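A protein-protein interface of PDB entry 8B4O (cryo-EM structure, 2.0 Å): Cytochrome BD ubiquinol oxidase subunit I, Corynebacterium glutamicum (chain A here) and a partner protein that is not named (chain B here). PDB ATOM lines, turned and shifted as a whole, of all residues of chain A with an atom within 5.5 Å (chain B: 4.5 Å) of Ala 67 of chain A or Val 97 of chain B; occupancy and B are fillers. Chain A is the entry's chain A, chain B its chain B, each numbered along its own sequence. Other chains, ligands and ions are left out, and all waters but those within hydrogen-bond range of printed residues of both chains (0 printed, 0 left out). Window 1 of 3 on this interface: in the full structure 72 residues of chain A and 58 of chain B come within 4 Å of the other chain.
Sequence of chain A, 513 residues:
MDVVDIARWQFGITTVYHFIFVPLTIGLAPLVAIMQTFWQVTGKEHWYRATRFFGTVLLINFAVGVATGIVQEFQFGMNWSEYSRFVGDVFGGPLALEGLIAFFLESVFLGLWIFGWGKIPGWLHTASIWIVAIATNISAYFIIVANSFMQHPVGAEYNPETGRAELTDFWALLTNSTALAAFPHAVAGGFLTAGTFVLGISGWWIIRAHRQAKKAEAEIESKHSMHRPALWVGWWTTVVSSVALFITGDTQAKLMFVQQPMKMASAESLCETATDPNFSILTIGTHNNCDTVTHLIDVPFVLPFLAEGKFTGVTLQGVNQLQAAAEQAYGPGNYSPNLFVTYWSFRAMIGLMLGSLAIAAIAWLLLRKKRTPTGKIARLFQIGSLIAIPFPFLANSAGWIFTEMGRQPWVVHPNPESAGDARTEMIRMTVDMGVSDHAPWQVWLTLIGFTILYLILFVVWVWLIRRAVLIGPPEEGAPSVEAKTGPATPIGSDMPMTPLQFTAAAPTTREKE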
ATOM      1  N   ALA A  63      -9.363 -18.296   6.744  1.00  0.00           N
ATOM      2  CA  ALA A  63      -8.270 -17.735   7.573  1.00  0.00           C
ATOM      3  C   ALA A  63      -7.089 -17.305   6.690  1.00  0.00           C
ATOM      4  O   ALA A  63      -6.701 -16.127   6.767  1.00  0.00           O
ATOM      5  CB  ALA A  63      -7.846 -18.744   8.607  1.00  0.00           C
ATOM      6  N   VAL A  64      -6.537 -18.224   5.896  1.00  0.00           N
ATOM      7  CA  VAL A  64      -5.351 -17.919   5.040  1.00  0.00           C
ATOM      8  C   VAL A  64      -5.738 -16.914   3.949  1.00  0.00           C
ATOM      9  O   VAL A  64      -4.841 -16.197   3.471  1.00  0.00           O
ATOM     10  CB  VAL A  64      -4.753 -19.203   4.430  1.00  0.00           C
ATOM     11  CG1 VAL A  64      -3.622 -18.900   3.462  1.00  0.00           C
ATOM     12  CG2 VAL A  64      -4.304 -20.185   5.502  1.00  0.00           C
ATOM     13  N   GLY A  65      -7.014 -16.879   3.561  1.00  0.00           N
ATOM     14  CA  GLY A  65      -7.480 -15.939   2.525  1.00  0.00           C
ATOM     15  C   GLY A  65      -7.403 -14.497   2.987  1.00  0.00           C
ATOM     16  O   GLY A  65      -7.186 -13.621   2.137  1.00  0.00           O
ATOM     17  N   VAL A  66      -7.572 -14.255   4.289  1.00  0.00           N
ATOM     18  CA  VAL A  66      -7.586 -12.860   4.819  1.00  0.00           C
ATOM     19  C   VAL A  66      -6.169 -12.279   4.846  1.00  0.00           C
ATOM     20  O   VAL A  66      -6.021 -11.116   4.433  1.00  0.00           O
ATOM     21  CB  VAL A  66      -8.231 -12.796   6.218  1.00  0.00           C
ATOM     22  CG1 VAL A  66      -8.033 -11.439   6.875  1.00  0.00           C
ATOM     23  CG2 VAL A  66      -9.706 -13.166   6.182  1.00  0.00           C
ATOM     24  N   ALA A  67      -5.160 -13.052   5.264  1.00  0.00           N
ATOM     25  CA  ALA A  67      -3.822 -12.481   5.436  1.00  0.00           C
ATOM     26  C   ALA A  67      -3.191 -12.102   4.099  1.00  0.00           C
ATOM     27  O   ALA A  67      -2.661 -10.984   3.922  1.00  0.00           O
ATOM     28  CB  ALA A  67      -2.938 -13.477   6.178  1.00  0.00           C
ATOM     29  N   THR A  68      -3.220 -13.037   3.151  1.00  0.00           N
ATOM     30  CA  THR A  68      -2.732 -12.748   1.813  1.00  0.00           C
ATOM     31  C   THR A  68      -3.457 -11.542   1.232  1.00  0.00           C
ATOM     32  O   THR A  68      -2.839 -10.681   0.578  1.00  0.00           O
ATOM     33  CB  THR A  68      -2.902 -13.991   0.938  1.00  0.00           C
ATOM     34  OG1 THR A  68      -4.281 -14.372   0.906  1.00  0.00           O
ATOM     35  CG2 THR A  68      -2.117 -15.156   1.504  1.00  0.00           C
ATOM     36  N   GLY A  69      -4.755 -11.422   1.522  1.00  0.00           N
ATOM     37  CA  GLY A  69      -5.472 -10.243   1.083  1.00  0.00           C
ATOM     38  C   GLY A  69      -4.886  -8.952   1.621  1.00  0.00           C
ATOM     39  O   GLY A  69      -4.695  -7.993   0.871  1.00  0.00           O
ATOM     40  N   ILE A  70      -4.607  -8.939   2.927  1.00  0.00           N
ATOM     41  CA  ILE A  70      -4.055  -7.741   3.628  1.00  0.00           C
ATOM     42  C   ILE A  70      -2.821  -7.211   2.888  1.00  0.00           C
ATOM     43  O   ILE A  70      -2.797  -6.007   2.573  1.00  0.00           O
ATOM     44  CB  ILE A  70      -3.733  -8.077   5.098  1.00  0.00           C
ATOM     45  CG1 ILE A  70      -4.970  -8.569   5.851  1.00  0.00           C
ATOM     46  CG2 ILE A  70      -3.085  -6.889   5.790  1.00  0.00           C
ATOM     47  CD1 ILE A  70      -4.699  -8.963   7.283  1.00  0.00           C
ATOM     48  N   VAL A  71      -1.847  -8.084   2.613  1.00  0.00           N
ATOM     49  CA  VAL A  71      -0.575  -7.671   1.950  1.00  0.00           C
ATOM     50  C   VAL A  71      -0.886  -7.053   0.586  1.00  0.00           C
ATOM     51  O   VAL A  71      -0.303  -5.998   0.280  1.00  0.00           O
ATOM     52  CB  VAL A  71       0.386  -8.865   1.804  1.00  0.00           C
ATOM     53  CG1 VAL A  71       1.590  -8.522   0.941  1.00  0.00           C
ATOM     54  CG2 VAL A  71       0.825  -9.401   3.156  1.00  0.00           C
ATOM     55  N   GLN A  72      -1.778  -7.670  -0.192  1.00  0.00           N
ATOM     56  CA  GLN A  72      -2.039  -7.181  -1.573  1.00  0.00           C
ATOM     57  C   GLN A  72      -2.448  -5.705  -1.539  1.00  0.00           C
ATOM     58  O   GLN A  72      -1.909  -4.932  -2.353  1.00  0.00           O
ATOM     59  CB  GLN A  72      -3.123  -8.025  -2.248  1.00  0.00           C
ATOM     60  CG  GLN A  72      -2.926  -9.524  -2.083  1.00  0.00           C
ATOM     61  CD  GLN A  72      -1.531  -9.976  -2.439  1.00  0.00           C
ATOM     62  OE1 GLN A  72      -0.869  -9.403  -3.302  1.00  0.00           O
ATOM     63  NE2 GLN A  72      -1.074 -11.023  -1.772  1.00  0.00           N
ATOM     64  N   TYR A 454       4.535 -17.713   3.342  1.00  0.00           N
ATOM     65  CA  TYR A 454       3.395 -18.257   2.619  1.00  0.00           C
ATOM     66  C   TYR A 454       3.546 -19.746   2.373  1.00  0.00           C
ATOM     67  O   TYR A 454       2.554 -20.479   2.368  1.00  0.00           O
ATOM     68  CB  TYR A 454       3.215 -17.520   1.298  1.00  0.00           C
ATOM     69  CG  TYR A 454       2.515 -16.207   1.468  1.00  0.00           C
ATOM     70  CD1 TYR A 454       1.856 -15.907   2.648  1.00  0.00           C
ATOM     71  CD2 TYR A 454       2.501 -15.272   0.451  1.00  0.00           C
ATOM     72  CE1 TYR A 454       1.219 -14.716   2.812  1.00  0.00           C
ATOM     73  CE2 TYR A 454       1.861 -14.078   0.608  1.00  0.00           C
ATOM     74  CZ  TYR A 454       1.222 -13.809   1.787  1.00  0.00           C
ATOM     75  OH  TYR A 454       0.577 -12.622   1.943  1.00  0.00           O
ATOM     76  N   LEU A 457       2.501 -21.317   5.554  1.00  0.00           N
ATOM     77  CA  LEU A 457       1.053 -21.254   5.732  1.00  0.00           C
ATOM     78  C   LEU A 457       0.336 -22.254   4.833  1.00  0.00           C
ATOM     79  O   LEU A 457      -0.604 -22.923   5.267  1.00  0.00           O
ATOM     80  CB  LEU A 457       0.545 -19.840   5.470  1.00  0.00           C
ATOM     81  CG  LEU A 457       1.033 -18.762   6.428  1.00  0.00           C
ATOM     82  CD1 LEU A 457       0.286 -17.480   6.155  1.00  0.00           C
ATOM     83  CD2 LEU A 457       0.866 -19.204   7.864  1.00  0.00           C
ATOM     84  N   TRP B  53     -12.421  -9.478  15.665  1.00  0.00           N
ATOM     85  CA  TRP B  53     -11.098  -8.920  15.422  1.00  0.00           C
ATOM     86  C   TRP B  53     -10.910  -8.761  13.923  1.00  0.00           C
ATOM     87  O   TRP B  53     -10.101  -7.949  13.466  1.00  0.00           O
ATOM     88  CB  TRP B  53      -9.999  -9.800  16.034  1.00  0.00           C
ATOM     89  CG  TRP B  53      -9.703 -11.064  15.270  1.00  0.00           C
ATOM     90  CD1 TRP B  53     -10.187 -12.305  15.535  1.00  0.00           C
ATOM     91  CD2 TRP B  53      -8.845 -11.204  14.129  1.00  0.00           C
ATOM     92  NE1 TRP B  53      -9.699 -13.208  14.628  1.00  0.00           N
ATOM     93  CE2 TRP B  53      -8.872 -12.557  13.753  1.00  0.00           C
ATOM     94  CE3 TRP B  53      -8.064 -10.314  13.385  1.00  0.00           C
ATOM     95  CZ2 TRP B  53      -8.147 -13.044  12.670  1.00  0.00           C
ATOM     96  CZ3 TRP B  53      -7.349 -10.798  12.309  1.00  0.00           C
ATOM     97  CH2 TRP B  53      -7.394 -12.150  11.961  1.00  0.00           C
ATOM     98  N   LEU B  93       1.079  -9.133  10.941  1.00  0.00           N
ATOM     99  CA  LEU B  93      -0.370  -9.246  10.808  1.00  0.00           C
ATOM    100  C   LEU B  93      -0.777 -10.583  10.200  1.00  0.00           C
ATOM    101  O   LEU B  93      -1.765 -11.183  10.627  1.00  0.00           O
ATOM    102  CB  LEU B  93      -0.916  -8.088   9.980  1.00  0.00           C
ATOM    103  CG  LEU B  93      -1.039  -6.761  10.722  1.00  0.00           C
ATOM    104  CD1 LEU B  93      -1.612  -5.703   9.806  1.00  0.00           C
ATOM    105  CD2 LEU B  93      -1.885  -6.919  11.970  1.00  0.00           C
ATOM    106  N   ILE B  94      -0.033 -11.061   9.203  1.00  0.00           N
ATOM    107  CA  ILE B  94      -0.275 -12.393   8.647  1.00  0.00           C
ATOM    108  C   ILE B  94      -0.138 -13.455   9.729  1.00  0.00           C
ATOM    109  O   ILE B  94      -0.994 -14.349   9.878  1.00  0.00           O
ATOM    110  CB  ILE B  94       0.709 -12.666   7.497  1.00  0.00           C
ATOM    111  CG1 ILE B  94       0.631 -11.586   6.428  1.00  0.00           C
ATOM    112  CG2 ILE B  94       0.481 -14.035   6.915  1.00  0.00           C
ATOM    113  CD1 ILE B  94       1.851 -11.562   5.555  1.00  0.00           C
ATOM    114  N   ILE B  95       0.963 -13.388  10.481  1.00  0.00           N
ATOM    115  CA  ILE B  95       1.216 -14.381  11.516  1.00  0.00           C
ATOM    116  C   ILE B  95       0.117 -14.342  12.572  1.00  0.00           C
ATOM    117  O   ILE B  95      -0.337 -15.385  13.053  1.00  0.00           O
ATOM    118  CB  ILE B  95       2.622 -14.171  12.111  1.00  0.00           C
ATOM    119  CG1 ILE B  95       3.691 -14.385  11.043  1.00  0.00           C
ATOM    120  CG2 ILE B  95       2.902 -15.145  13.194  1.00  0.00           C
ATOM    121  CD1 ILE B  95       5.076 -13.953  11.475  1.00  0.00           C
ATOM    122  N   ARG B  96      -0.365 -13.146  12.917  1.00  0.00           N
ATOM    123  CA  ARG B  96      -1.469 -13.042  13.866  1.00  0.00           C
ATOM    124  C   ARG B  96      -2.769 -13.582  13.284  1.00  0.00           C
ATOM    125  O   ARG B  96      -3.565 -14.189  14.004  1.00  0.00           O
ATOM    126  CB  ARG B  96      -1.661 -11.595  14.305  1.00  0.00           C
ATOM    127  CG  ARG B  96      -2.684 -11.435  15.412  1.00  0.00           C
ATOM    128  CD  ARG B  96      -2.783  -9.999  15.867  1.00  0.00           C
ATOM    129  NE  ARG B  96      -3.328  -9.138  14.824  1.00  0.00           N
ATOM    130  CZ  ARG B  96      -4.538  -8.597  14.857  1.00  0.00           C
ATOM    131  NH1 ARG B  96      -5.338  -8.819  15.888  1.00  0.00           N
ATOM    132  NH2 ARG B  96      -4.946  -7.829  13.861  1.00  0.00           N
ATOM    133  N   VAL B  97      -3.012 -13.358  11.992  1.00  0.00           N
ATOM    134  CA  VAL B  97      -4.233 -13.861  11.369  1.00  0.00           C
ATOM    135  C   VAL B  97      -4.310 -15.371  11.524  1.00  0.00           C
ATOM    136  O   VAL B  97      -5.318 -15.921  11.992  1.00  0.00           O
ATOM    137  CB  VAL B  97      -4.297 -13.455   9.886  1.00  0.00           C
ATOM    138  CG1 VAL B  97      -5.310 -14.310   9.150  1.00  0.00           C
ATOM    139  CG2 VAL B  97      -4.651 -11.991   9.743  1.00  0.00           C
ATOM    140  N   VAL B  98      -3.229 -16.063  11.160  1.00  0.00           N
ATOM    141  CA  VAL B  98      -3.261 -17.520  11.280  1.00  0.00           C
ATOM    142  C   VAL B  98      -3.278 -17.941  12.747  1.00  0.00           C
ATOM    143  O   VAL B  98      -4.030 -18.842  13.131  1.00  0.00           O
ATOM    144  CB  VAL B  98      -2.109 -18.171  10.494  1.00  0.00           C
ATOM    145  CG1 VAL B  98      -2.299 -17.926   9.013  1.00  0.00           C
ATOM    146  CG2 VAL B  98      -0.765 -17.645  10.946  1.00  0.00           C
ATOM    147  N   GLY B  99      -2.503 -17.263  13.600  1.00  0.00           N
ATOM    148  CA  GLY B  99      -2.456 -17.646  15.002  1.00  0.00           C
ATOM    149  C   GLY B  99      -3.791 -17.506  15.706  1.00  0.00           C
ATOM    150  O   GLY B  99      -4.084 -18.240  16.649  1.00  0.00           O
ATOM    151  N   LEU B 100      -4.613 -16.553  15.268  1.00  0.00           N
ATOM    152  CA  LEU B 100      -5.923 -16.376  15.877  1.00  0.00           C
ATOM    153  C   LEU B 100      -6.977 -17.284  15.261  1.00  0.00           C
ATOM    154  O   LEU B 100      -7.769 -17.882  15.994  1.00  0.00           O
ATOM    155  CB  LEU B 100      -6.377 -14.920  15.764  1.00  0.00           C
ATOM    156  CG  LEU B 100      -5.580 -13.845  16.495  1.00  0.00           C
ATOM    157  CD1 LEU B 100      -6.087 -12.477  16.096  1.00  0.00           C
ATOM    158  CD2 LEU B 100      -5.685 -14.034  17.988  1.00  0.00           C
ATOM    159  N   GLU B 101      -7.017 -17.403  13.933  1.00  0.00           N
ATOM    160  CA  GLU B 101      -8.084 -18.191  13.326  1.00  0.00           C
ATOM    161  C   GLU B 101      -7.855 -19.691  13.480  1.00  0.00           C
ATOM    162  O   GLU B 101      -8.781 -20.435  13.815  1.00  0.00           O
ATOM    163  CB  GLU B 101      -8.252 -17.812  11.857  1.00  0.00           C
ATOM    164  CG  GLU B 101      -8.751 -16.398  11.632  1.00  0.00           C
ATOM    165  CD  GLU B 101     -10.169 -16.197  12.127  1.00  0.00           C
ATOM    166  OE1 GLU B 101     -10.961 -17.158  12.083  1.00  0.00           O
ATOM    167  OE2 GLU B 101     -10.499 -15.076  12.562  1.00  0.00           O
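Among the printed residues, pairs that only touch across the chains: Ala 63 of chain A with Val 97 of chain B (3.3 Å), Ala 63 of chain A with Glu 101 of chain B (3.4 Å), Ala 67 of chain A with Ile 94 of chain B (3.5 Å), Ala 67 of chain A with Val 97 of chain B (3.9 Å), Ile 70 of chain A with Val 97 of chain B (3.9 Å), Val 71 of chain A with Ile 94 of chain B (3.4 Å), Tyr 454 of chain A with Ile 94 of chain B (3.97 Å), Leu 457 of chain A with Ile 94 of chain B (3.5 Å) and Leu 457 of chain A with Val 98 of chain B (3.6 Å).
The side-chain carboxylate (OE2) of Glu 101 of chain B is in hydrogen-bond range of the indole nitrogen (NE1) of Trp 53 of chain B (2.9 Å).
Of the 10 printed residues of chain B, 4 touch a printed residue of chain A.
Hydrophobic or aromatic side chains of chain B within 4 Å of the printed part of chain A: Ile 94, Val 97 and Val 98.
Of the 12 printed residues of chain A, 6 touch a printed residue of chain B.
Printed residues of chain A that touch a printed residue of chain B: Ala 63, Ala 67, Ile 70, Val 71, Tyr 454 and Leu 457.
Hydrophobic or aromatic side chains of chain A that line the printed part of chain B: Ala 63, Ala 67, Ile 70, Val 71, Tyr 454 and Leu 457.
Among the printed residues, 9 pairs touch across the chains.
Val 66 of chain A touches none of the printed residues of chain B.
Ala 67 of chain A touches just these residues of chain B: Ile 94 (3.5 Å) and Val 97 (3.9 Å).
Of the printed residues of chain B, Tyr 454 of chain A touches Ile 94.
Of the printed residues of chain B, Leu 457 of chain A touches Ile 94 and Val 98.
Trp 53 of chain B touches none of the printed residues of chain A.
Printed residues of chain A within 4 Å of Ile 94 of chain B: Ala 67 (3.5 Å), Val 71 (3.4 Å), Tyr 454 (3.97 Å) and Leu 457 (3.5 Å).
Of the printed residues of chain A, Val 98 of chain B touches Leu 457.
Of the printed residues of chain A, Glu 101 of chain B touches Ala 63.
The nearest residue of chain A that does not touch Val 97 of chain B is Val 66 of chain A (4.4 Å).
The nearest printed residue of chain A that does not touch Val 98 of chain B is Val 64 of chain A (4.6 Å).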
